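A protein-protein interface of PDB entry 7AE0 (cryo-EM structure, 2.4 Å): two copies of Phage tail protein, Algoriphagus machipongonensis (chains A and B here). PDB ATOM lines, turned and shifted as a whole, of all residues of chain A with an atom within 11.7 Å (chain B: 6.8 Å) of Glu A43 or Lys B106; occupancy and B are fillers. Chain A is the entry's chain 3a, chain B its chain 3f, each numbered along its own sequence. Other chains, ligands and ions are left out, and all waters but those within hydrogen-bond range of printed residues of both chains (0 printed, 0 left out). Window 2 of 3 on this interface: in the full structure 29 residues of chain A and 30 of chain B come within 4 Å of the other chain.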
ATOM      1  N   ILE A  33     -27.072 -13.684  11.371  1.00  0.00           N
ATOM      2  CA  ILE A  33     -26.737 -12.952  12.596  1.00  0.00           C
ATOM      3  C   ILE A  33     -25.232 -12.845  12.790  1.00  0.00           C
ATOM      4  O   ILE A  33     -24.515 -13.772  12.471  1.00  0.00           O
ATOM      5  CB  ILE A  33     -27.273 -13.630  13.867  1.00  0.00           C
ATOM      6  CG1 ILE A  33     -28.761 -13.851  13.831  1.00  0.00           C
ATOM      7  CG2 ILE A  33     -27.026 -12.773  15.093  1.00  0.00           C
ATOM      8  CD1 ILE A  33     -29.301 -14.323  15.161  1.00  0.00           C
ATOM      9  N   TYR A  36     -21.273 -10.721  19.094  1.00  0.00           N
ATOM     10  CA  TYR A  36     -20.072 -10.128  19.713  1.00  0.00           C
ATOM     11  C   TYR A  36     -20.079  -9.996  21.254  1.00  0.00           C
ATOM     12  O   TYR A  36     -21.105  -9.691  21.859  1.00  0.00           O
ATOM     13  CB  TYR A  36     -19.861  -8.737  19.103  1.00  0.00           C
ATOM     14  CG  TYR A  36     -18.663  -7.961  19.591  1.00  0.00           C
ATOM     15  CD1 TYR A  36     -17.421  -8.155  19.024  1.00  0.00           C
ATOM     16  CD2 TYR A  36     -18.794  -7.033  20.610  1.00  0.00           C
ATOM     17  CE1 TYR A  36     -16.341  -7.437  19.465  1.00  0.00           C
ATOM     18  CE2 TYR A  36     -17.720  -6.320  21.054  1.00  0.00           C
ATOM     19  CZ  TYR A  36     -16.497  -6.517  20.482  1.00  0.00           C
ATOM     20  OH  TYR A  36     -15.415  -5.800  20.919  1.00  0.00           O
ATOM     21  N   ARG A  37     -18.917 -10.216  21.898  1.00  0.00           N
ATOM     22  CA  ARG A  37     -18.759  -9.927  23.336  1.00  0.00           C
ATOM     23  C   ARG A  37     -17.344  -9.478  23.697  1.00  0.00           C
ATOM     24  O   ARG A  37     -16.376 -10.180  23.409  1.00  0.00           O
ATOM     25  CB  ARG A  37     -19.115 -11.127  24.229  1.00  0.00           C
ATOM     26  CG  ARG A  37     -18.915 -10.829  25.732  1.00  0.00           C
ATOM     27  CD  ARG A  37     -19.306 -11.912  26.702  1.00  0.00           C
ATOM     28  NE  ARG A  37     -19.019 -11.442  28.079  1.00  0.00           N
ATOM     29  CZ  ARG A  37     -17.834 -11.575  28.728  1.00  0.00           C
ATOM     30  NH1 ARG A  37     -16.829 -12.218  28.162  1.00  0.00           N
ATOM     31  NH2 ARG A  37     -17.637 -11.056  29.940  1.00  0.00           N
ATOM     32  N   HIS A  38     -17.190  -8.304  24.307  1.00  0.00           N
ATOM     33  CA  HIS A  38     -15.840  -7.988  24.797  1.00  0.00           C
ATOM     34  C   HIS A  38     -15.713  -8.517  26.232  1.00  0.00           C
ATOM     35  O   HIS A  38     -16.701  -8.609  26.966  1.00  0.00           O
ATOM     36  CB  HIS A  38     -15.448  -6.505  24.629  1.00  0.00           C
ATOM     37  CG  HIS A  38     -16.138  -5.605  25.581  1.00  0.00           C
ATOM     38  ND1 HIS A  38     -15.722  -5.448  26.879  1.00  0.00           N
ATOM     39  CD2 HIS A  38     -17.259  -4.870  25.449  1.00  0.00           C
ATOM     40  CE1 HIS A  38     -16.543  -4.630  27.499  1.00  0.00           C
ATOM     41  NE2 HIS A  38     -17.487  -4.271  26.655  1.00  0.00           N
ATOM     42  N   GLY A  39     -14.473  -8.834  26.607  1.00  0.00           N
ATOM     43  CA  GLY A  39     -14.126  -9.475  27.875  1.00  0.00           C
ATOM     44  C   GLY A  39     -14.536  -8.755  29.156  1.00  0.00           C
ATOM     45  O   GLY A  39     -14.779  -9.406  30.171  1.00  0.00           O
ATOM     46  N   ALA A  40     -14.621  -7.427  29.137  1.00  0.00           N
ATOM     47  CA  ALA A  40     -14.985  -6.683  30.336  1.00  0.00           C
ATOM     48  C   ALA A  40     -16.488  -6.564  30.587  1.00  0.00           C
ATOM     49  O   ALA A  40     -16.875  -5.953  31.583  1.00  0.00           O
ATOM     50  CB  ALA A  40     -14.395  -5.288  30.267  1.00  0.00           C
ATOM     51  N   SER A  41     -17.343  -7.081  29.714  1.00  0.00           N
ATOM     52  CA  SER A  41     -18.781  -6.920  29.918  1.00  0.00           C
ATOM     53  C   SER A  41     -19.306  -7.659  31.169  1.00  0.00           C
ATOM     54  O   SER A  41     -18.952  -8.813  31.394  1.00  0.00           O
ATOM     55  CB  SER A  41     -19.545  -7.424  28.716  1.00  0.00           C
ATOM     56  OG  SER A  41     -20.932  -7.374  28.968  1.00  0.00           O
ATOM     57  N   PRO A  42     -20.172  -7.008  31.978  1.00  0.00           N
ATOM     58  CA  PRO A  42     -20.898  -7.616  33.115  1.00  0.00           C
ATOM     59  C   PRO A  42     -21.845  -8.746  32.731  1.00  0.00           C
ATOM     60  O   PRO A  42     -22.281  -9.505  33.600  1.00  0.00           O
ATOM     61  CB  PRO A  42     -21.707  -6.426  33.660  1.00  0.00           C
ATOM     62  CG  PRO A  42     -20.976  -5.225  33.216  1.00  0.00           C
ATOM     63  CD  PRO A  42     -20.372  -5.566  31.892  1.00  0.00           C
ATOM     64  N   GLU A  43     -22.242  -8.829  31.469  1.00  0.00           N
ATOM     65  CA  GLU A  43     -23.124  -9.901  31.045  1.00  0.00           C
ATOM     66  C   GLU A  43     -22.294 -10.972  30.381  1.00  0.00           C
ATOM     67  O   GLU A  43     -21.333 -10.677  29.673  1.00  0.00           O
ATOM     68  CB  GLU A  43     -24.218  -9.420  30.095  1.00  0.00           C
ATOM     69  CG  GLU A  43     -25.224  -8.505  30.728  1.00  0.00           C
ATOM     70  CD  GLU A  43     -26.347  -8.133  29.794  1.00  0.00           C
ATOM     71  OE1 GLU A  43     -26.222  -8.386  28.610  1.00  0.00           O
ATOM     72  OE2 GLU A  43     -27.343  -7.608  30.252  1.00  0.00           O
ATOM     73  N   TYR A  44     -22.715 -12.208  30.548  1.00  0.00           N
ATOM     74  CA  TYR A  44     -21.960 -13.338  30.039  1.00  0.00           C
ATOM     75  C   TYR A  44     -22.617 -13.979  28.826  1.00  0.00           C
ATOM     76  O   TYR A  44     -22.597 -15.194  28.652  1.00  0.00           O
ATOM     77  CB  TYR A  44     -21.723 -14.315  31.179  1.00  0.00           C
ATOM     78  CG  TYR A  44     -21.106 -13.592  32.371  1.00  0.00           C
ATOM     79  CD1 TYR A  44     -21.753 -13.577  33.586  1.00  0.00           C
ATOM     80  CD2 TYR A  44     -19.925 -12.874  32.240  1.00  0.00           C
ATOM     81  CE1 TYR A  44     -21.238 -12.892  34.649  1.00  0.00           C
ATOM     82  CE2 TYR A  44     -19.410 -12.178  33.302  1.00  0.00           C
ATOM     83  CZ  TYR A  44     -20.068 -12.193  34.508  1.00  0.00           C
ATOM     84  OH  TYR A  44     -19.560 -11.508  35.578  1.00  0.00           O
ATOM     85  N   SER A  45     -23.191 -13.130  27.983  1.00  0.00           N
ATOM     86  CA  SER A  45     -23.847 -13.510  26.749  1.00  0.00           C
ATOM     87  C   SER A  45     -23.478 -12.485  25.680  1.00  0.00           C
ATOM     88  O   SER A  45     -22.849 -11.468  25.975  1.00  0.00           O
ATOM     89  CB  SER A  45     -25.348 -13.589  26.952  1.00  0.00           C
ATOM     90  OG  SER A  45     -25.869 -12.329  27.256  1.00  0.00           O
ATOM     91  N   LYS A  46     -23.835 -12.753  24.429  1.00  0.00           N
ATOM     92  CA  LYS A  46     -23.438 -11.896  23.313  1.00  0.00           C
ATOM     93  C   LYS A  46     -24.506 -10.917  22.819  1.00  0.00           C
ATOM     94  O   LYS A  46     -25.704 -11.137  22.981  1.00  0.00           O
ATOM     95  CB  LYS A  46     -22.997 -12.787  22.160  1.00  0.00           C
ATOM     96  CG  LYS A  46     -21.774 -13.605  22.502  1.00  0.00           C
ATOM     97  CD  LYS A  46     -21.373 -14.495  21.388  1.00  0.00           C
ATOM     98  CE  LYS A  46     -20.188 -15.337  21.759  1.00  0.00           C
ATOM     99  NZ  LYS A  46     -19.833 -16.275  20.668  1.00  0.00           N
ATOM    100  N   ILE A  47     -24.044  -9.846  22.156  1.00  0.00           N
ATOM    101  CA  ILE A  47     -24.928  -8.869  21.514  1.00  0.00           C
ATOM    102  C   ILE A  47     -25.074  -9.244  20.045  1.00  0.00           C
ATOM    103  O   ILE A  47     -24.134  -9.747  19.424  1.00  0.00           O
ATOM    104  CB  ILE A  47     -24.440  -7.410  21.694  1.00  0.00           C
ATOM    105  CG1 ILE A  47     -23.054  -7.175  21.054  1.00  0.00           C
ATOM    106  CG2 ILE A  47     -24.424  -7.096  23.184  1.00  0.00           C
ATOM    107  CD1 ILE A  47     -22.620  -5.738  20.954  1.00  0.00           C
ATOM    108  N   LYS A  48     -26.271  -9.062  19.490  1.00  0.00           N
ATOM    109  CA  LYS A  48     -26.542  -9.496  18.121  1.00  0.00           C
ATOM    110  C   LYS A  48     -26.914  -8.385  17.134  1.00  0.00           C
ATOM    111  O   LYS A  48     -27.682  -7.485  17.470  1.00  0.00           O
ATOM    112  CB  LYS A  48     -27.680 -10.491  18.192  1.00  0.00           C
ATOM    113  CG  LYS A  48     -27.337 -11.680  19.043  1.00  0.00           C
ATOM    114  CD  LYS A  48     -28.454 -12.655  19.167  1.00  0.00           C
ATOM    115  CE  LYS A  48     -28.043 -13.785  20.086  1.00  0.00           C
ATOM    116  NZ  LYS A  48     -29.120 -14.776  20.268  1.00  0.00           N
ATOM    117  N   MET A  49     -26.446  -8.503  15.885  1.00  0.00           N
ATOM    118  CA  MET A  49     -26.848  -7.584  14.815  1.00  0.00           C
ATOM    119  C   MET A  49     -27.015  -8.306  13.462  1.00  0.00           C
ATOM    120  O   MET A  49     -26.375  -9.328  13.233  1.00  0.00           O
ATOM    121  CB  MET A  49     -25.828  -6.441  14.686  1.00  0.00           C
ATOM    122  CG  MET A  49     -24.471  -6.859  14.226  1.00  0.00           C
ATOM    123  SD  MET A  49     -23.337  -5.474  14.143  1.00  0.00           S
ATOM    124  CE  MET A  49     -21.920  -6.256  13.411  1.00  0.00           C
ATOM    125  N   MET B  52     -20.712 -19.725  30.423  1.00  0.00           N
ATOM    126  CA  MET B  52     -21.430 -18.655  29.724  1.00  0.00           C
ATOM    127  C   MET B  52     -22.901 -19.004  29.426  1.00  0.00           C
ATOM    128  O   MET B  52     -23.291 -20.159  29.378  1.00  0.00           O
ATOM    129  CB  MET B  52     -20.678 -18.272  28.442  1.00  0.00           C
ATOM    130  CG  MET B  52     -19.184 -17.994  28.662  1.00  0.00           C
ATOM    131  SD  MET B  52     -18.362 -16.873  27.501  1.00  0.00           S
ATOM    132  CE  MET B  52     -19.221 -15.392  27.971  1.00  0.00           C
ATOM    133  N   ARG B  86     -37.264  -3.893  19.458  1.00  0.00           N
ATOM    134  CA  ARG B  86     -38.429  -3.691  20.315  1.00  0.00           C
ATOM    135  C   ARG B  86     -38.442  -4.512  21.606  1.00  0.00           C
ATOM    136  O   ARG B  86     -37.860  -5.594  21.710  1.00  0.00           O
ATOM    137  CB  ARG B  86     -39.710  -4.014  19.553  1.00  0.00           C
ATOM    138  CG  ARG B  86     -39.960  -3.175  18.305  1.00  0.00           C
ATOM    139  CD  ARG B  86     -41.254  -3.513  17.659  1.00  0.00           C
ATOM    140  NE  ARG B  86     -41.403  -2.824  16.395  1.00  0.00           N
ATOM    141  CZ  ARG B  86     -42.397  -2.999  15.522  1.00  0.00           C
ATOM    142  NH1 ARG B  86     -43.387  -3.845  15.764  1.00  0.00           N
ATOM    143  NH2 ARG B  86     -42.383  -2.304  14.392  1.00  0.00           N
ATOM    144  N   ASP B  87     -39.225  -4.018  22.559  1.00  0.00           N
ATOM    145  CA  ASP B  87     -39.431  -4.703  23.820  1.00  0.00           C
ATOM    146  C   ASP B  87     -40.658  -5.585  23.625  1.00  0.00           C
ATOM    147  O   ASP B  87     -41.731  -5.093  23.265  1.00  0.00           O
ATOM    148  CB  ASP B  87     -39.654  -3.708  24.955  1.00  0.00           C
ATOM    149  CG  ASP B  87     -38.474  -2.778  25.159  1.00  0.00           C
ATOM    150  OD1 ASP B  87     -37.452  -2.951  24.463  1.00  0.00           O
ATOM    151  OD2 ASP B  87     -38.565  -1.880  26.023  1.00  0.00           O
ATOM    152  N   LEU B  88     -40.496  -6.876  23.858  1.00  0.00           N
ATOM    153  CA  LEU B  88     -41.545  -7.868  23.660  1.00  0.00           C
ATOM    154  C   LEU B  88     -42.119  -8.361  24.992  1.00  0.00           C
ATOM    155  O   LEU B  88     -41.385  -8.878  25.839  1.00  0.00           O
ATOM    156  CB  LEU B  88     -40.956  -9.016  22.827  1.00  0.00           C
ATOM    157  CG  LEU B  88     -41.773 -10.299  22.586  1.00  0.00           C
ATOM    158  CD1 LEU B  88     -42.991 -10.014  21.739  1.00  0.00           C
ATOM    159  CD2 LEU B  88     -40.875 -11.343  21.930  1.00  0.00           C
ATOM    160  N   LYS B 104     -40.659 -11.299  30.004  1.00  0.00           N
ATOM    161  CA  LYS B 104     -40.148 -10.023  29.514  1.00  0.00           C
ATOM    162  C   LYS B 104     -38.910 -10.196  28.642  1.00  0.00           C
ATOM    163  O   LYS B 104     -37.886 -10.696  29.109  1.00  0.00           O
ATOM    164  CB  LYS B 104     -39.832  -9.129  30.700  1.00  0.00           C
ATOM    165  CG  LYS B 104     -41.047  -8.772  31.506  1.00  0.00           C
ATOM    166  CD  LYS B 104     -40.690  -7.922  32.682  1.00  0.00           C
ATOM    167  CE  LYS B 104     -41.915  -7.544  33.462  1.00  0.00           C
ATOM    168  NZ  LYS B 104     -41.578  -6.696  34.630  1.00  0.00           N
ATOM    169  N   VAL B 105     -38.987  -9.759  27.381  1.00  0.00           N
ATOM    170  CA  VAL B 105     -37.902  -9.947  26.419  1.00  0.00           C
ATOM    171  C   VAL B 105     -37.290  -8.630  25.913  1.00  0.00           C
ATOM    172  O   VAL B 105     -37.977  -7.755  25.371  1.00  0.00           O
ATOM    173  CB  VAL B 105     -38.395 -10.822  25.257  1.00  0.00           C
ATOM    174  CG1 VAL B 105     -37.333 -10.974  24.211  1.00  0.00           C
ATOM    175  CG2 VAL B 105     -38.778 -12.175  25.788  1.00  0.00           C
ATOM    176  N   LYS B 106     -35.973  -8.533  26.061  1.00  0.00           N
ATOM    177  CA  LYS B 106     -35.148  -7.376  25.702  1.00  0.00           C
ATOM    178  C   LYS B 106     -34.586  -7.382  24.261  1.00  0.00           C
ATOM    179  O   LYS B 106     -34.008  -8.373  23.818  1.00  0.00           O
ATOM    180  CB  LYS B 106     -33.990  -7.347  26.703  1.00  0.00           C
ATOM    181  CG  LYS B 106     -33.022  -6.208  26.601  1.00  0.00           C
ATOM    182  CD  LYS B 106     -32.038  -6.208  27.784  1.00  0.00           C
ATOM    183  CE  LYS B 106     -31.051  -7.386  27.709  1.00  0.00           C
ATOM    184  NZ  LYS B 106     -29.994  -7.312  28.729  1.00  0.00           N
ATOM    185  N   ASN B 107     -34.618  -6.223  23.601  1.00  0.00           N
ATOM    186  CA  ASN B 107     -33.968  -5.981  22.290  1.00  0.00           C
ATOM    187  C   ASN B 107     -34.271  -6.938  21.122  1.00  0.00           C
ATOM    188  O   ASN B 107     -33.357  -7.320  20.417  1.00  0.00           O
ATOM    189  CB  ASN B 107     -32.439  -5.908  22.460  1.00  0.00           C
ATOM    190  CG  ASN B 107     -31.940  -4.508  22.734  1.00  0.00           C
ATOM    191  OD1 ASN B 107     -32.645  -3.540  22.542  1.00  0.00           O
ATOM    192  ND2 ASN B 107     -30.717  -4.405  23.186  1.00  0.00           N
ATOM    193  N   ALA B 108     -35.525  -7.320  20.903  1.00  0.00           N
ATOM    194  CA  ALA B 108     -35.885  -8.235  19.822  1.00  0.00           C
ATOM    195  C   ALA B 108     -35.937  -7.600  18.430  1.00  0.00           C
ATOM    196  O   ALA B 108     -36.171  -6.419  18.300  1.00  0.00           O
ATOM    197  CB  ALA B 108     -37.201  -8.924  20.146  1.00  0.00           C
ATOM    198  N   TRP B 109     -35.634  -8.395  17.406  1.00  0.00           N
ATOM    199  CA  TRP B 109     -35.750  -8.026  15.996  1.00  0.00           C
ATOM    200  C   TRP B 109     -35.918  -9.319  15.184  1.00  0.00           C
ATOM    201  O   TRP B 109     -35.565 -10.388  15.656  1.00  0.00           O
ATOM    202  CB  TRP B 109     -34.581  -7.124  15.522  1.00  0.00           C
ATOM    203  CG  TRP B 109     -33.230  -7.704  15.706  1.00  0.00           C
ATOM    204  CD1 TRP B 109     -32.457  -7.611  16.812  1.00  0.00           C
ATOM    205  CD2 TRP B 109     -32.481  -8.463  14.758  1.00  0.00           C
ATOM    206  NE1 TRP B 109     -31.290  -8.267  16.629  1.00  0.00           N
ATOM    207  CE2 TRP B 109     -31.267  -8.803  15.375  1.00  0.00           C
ATOM    208  CE3 TRP B 109     -32.727  -8.904  13.456  1.00  0.00           C
ATOM    209  CZ2 TRP B 109     -30.294  -9.554  14.741  1.00  0.00           C
ATOM    210  CZ3 TRP B 109     -31.764  -9.631  12.822  1.00  0.00           C
ATOM    211  CH2 TRP B 109     -30.556  -9.954  13.465  1.00  0.00           C
ATOM    212  N   ALA B 133     -34.860 -12.856  17.192  1.00  0.00           N
ATOM    213  CA  ALA B 133     -33.626 -12.850  17.969  1.00  0.00           C
ATOM    214  C   ALA B 133     -33.814 -11.895  19.136  1.00  0.00           C
ATOM    215  O   ALA B 133     -34.573 -10.943  19.022  1.00  0.00           O
ATOM    216  CB  ALA B 133     -32.454 -12.405  17.108  1.00  0.00           C
ATOM    217  N   HIS B 134     -33.134 -12.130  20.255  1.00  0.00           N
ATOM    218  CA  HIS B 134     -33.244 -11.200  21.382  1.00  0.00           C
ATOM    219  C   HIS B 134     -32.015 -11.308  22.273  1.00  0.00           C
ATOM    220  O   HIS B 134     -31.148 -12.148  22.049  1.00  0.00           O
ATOM    221  CB  HIS B 134     -34.522 -11.443  22.171  1.00  0.00           C
ATOM    222  CG  HIS B 134     -34.569 -12.748  22.844  1.00  0.00           C
ATOM    223  ND1 HIS B 134     -34.166 -12.938  24.147  1.00  0.00           N
ATOM    224  CD2 HIS B 134     -34.934 -13.949  22.374  1.00  0.00           C
ATOM    225  CE1 HIS B 134     -34.306 -14.210  24.448  1.00  0.00           C
ATOM    226  NE2 HIS B 134     -34.757 -14.845  23.382  1.00  0.00           N
ATOM    227  N   GLU B 135     -31.931 -10.425  23.276  1.00  0.00           N
ATOM    228  CA  GLU B 135     -30.784 -10.390  24.184  1.00  0.00           C
ATOM    229  C   GLU B 135     -31.092 -10.682  25.662  1.00  0.00           C
ATOM    230  O   GLU B 135     -30.308 -10.286  26.528  1.00  0.00           O
ATOM    231  CB  GLU B 135     -30.074  -9.039  24.065  1.00  0.00           C
ATOM    232  CG  GLU B 135     -29.434  -8.797  22.693  1.00  0.00           C
ATOM    233  CD  GLU B 135     -28.702  -7.489  22.578  1.00  0.00           C
ATOM    234  OE1 GLU B 135     -28.787  -6.687  23.485  1.00  0.00           O
ATOM    235  OE2 GLU B 135     -28.052  -7.271  21.576  1.00  0.00           O
ATOM    236  N   GLY B 136     -32.185 -11.355  25.986  1.00  0.00           N
ATOM    237  CA  GLY B 136     -32.428 -11.647  27.388  1.00  0.00           C
ATOM    238  C   GLY B 136     -33.883 -11.786  27.783  1.00  0.00           C
ATOM    239  O   GLY B 136     -34.764 -11.084  27.285  1.00  0.00           O
ATOM    240  N   LEU B 137     -34.111 -12.678  28.749  1.00  0.00           N
ATOM    241  CA  LEU B 137     -35.430 -13.038  29.251  1.00  0.00           C
ATOM    242  C   LEU B 137     -35.520 -13.075  30.778  1.00  0.00           C
ATOM    243  O   LEU B 137     -34.723 -13.734  31.447  1.00  0.00           O
ATOM    244  CB  LEU B 137     -35.835 -14.408  28.670  1.00  0.00           C
ATOM    245  CG  LEU B 137     -37.105 -15.102  29.225  1.00  0.00           C
ATOM    246  CD1 LEU B 137     -38.339 -14.294  28.919  1.00  0.00           C
ATOM    247  CD2 LEU B 137     -37.235 -16.509  28.610  1.00  0.00           C
ATOM    248  N   VAL B 138     -36.537 -12.395  31.308  1.00  0.00           N
ATOM    249  CA  VAL B 138     -36.860 -12.372  32.736  1.00  0.00           C
ATOM    250  C   VAL B 138     -38.279 -12.906  32.966  1.00  0.00           C
ATOM    251  O   VAL B 138     -39.215 -12.534  32.252  1.00  0.00           O
ATOM    252  CB  VAL B 138     -36.701 -10.953  33.320  1.00  0.00           C
ATOM    253  CG1 VAL B 138     -37.116 -10.911  34.781  1.00  0.00           C
ATOM    254  CG2 VAL B 138     -35.261 -10.519  33.196  1.00  0.00           C
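Among the printed residues, merely in contact across the chains: Arg A37 with Met B52, Tyr A44 with Met B52, Ile A47 with Glu B135, Lys A48 with Trp B109, Lys A48 with His B134 and Met A49 with Trp B109.
No position is printed for both chains. Of the 8 pairs that touch across the chains among the printed residues, none has its exchanged pair printed and touching as well.
The side-chain carboxylate of Glu A43 lies within salt-bridge range of the side-chain amino group of Lys B106, at 3.1 Å. N of Lys A48 is in hydrogen-bond range of OE2 of Glu B135 (3.3 Å).
Printed residues of chain A that touch a printed residue of chain B: Arg A37, Glu A43, Tyr A44, Ile A47, Lys A48 and Met A49. Hydrophobic or aromatic side chains of chain A that line the printed part of chain B: Ile A47. Among the printed residues, 8 pairs touch across the chains.
Of the printed residues of chain B, Arg A37 touches Met B52 (3.7 Å). Of chain B, only Lys B106 (3.1 Å) comes within 4 Å of Glu A43. Printed residues of chain B within 4 Å of Tyr A44: Met B52 (3.4 Å). Lys A46 touches none of the printed residues of chain B. Of the printed residues of chain B, Ile A47 touches Glu B135 (3.5 Å). Printed residues of chain B within 4 Å of Lys A48: Trp B109 (3.8 Å), His B134 (3.8 Å) and Glu B135 (3.3 Å). Of the printed residues of chain B, Met A49 touches Trp B109 (3.7 Å). Val B105 touches none of the printed residues of chain A. Printed residues of chain A within 4 Å of Lys B106: Glu A43 (3.1 Å). No residue of chain A comes within 4 Å of Asn B107. Ala B133 touches none of the printed residues of chain A. Of chain A, only Ile A47 (3.5 Å) and Lys A48 (3.3 Å) come within 4 Å of Glu B135. No residue of chain A comes within 4 Å of Gly B136. The nearest residue of chain B that does not touch Glu A43 is Glu B135 (5.0 Å). The nearest printed residue of chain B that does not touch Lys A48 is Ala B133 (4.5 Å).
The backbone carbonyl oxygen of Ser A41 is in hydrogen-bond range of the guanidinium group of Arg A37. NE of Arg A37 sits at hydrogen-bond distance from O of Glu A43, 2.9 Å away. The backbone carbonyl oxygen of Gly B136 lies within hydrogen-bond range of the backbone NH of Lys B106, 3.1 Å away. The side-chain carboxylate of Glu B135 sits at hydrogen-bond distance from the side-chain amide nitrogen of Asn B107 (3.0 Å). The backbone carbonyl oxygen (O) of Trp B109 is in hydrogen-bond range of the backbone NH (N) of Ala B133 (3.0 Å). A ring nitrogen (ND1) of His B134 lies within hydrogen-bond range of the backbone NH of Gly B136 (3.1 Å).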
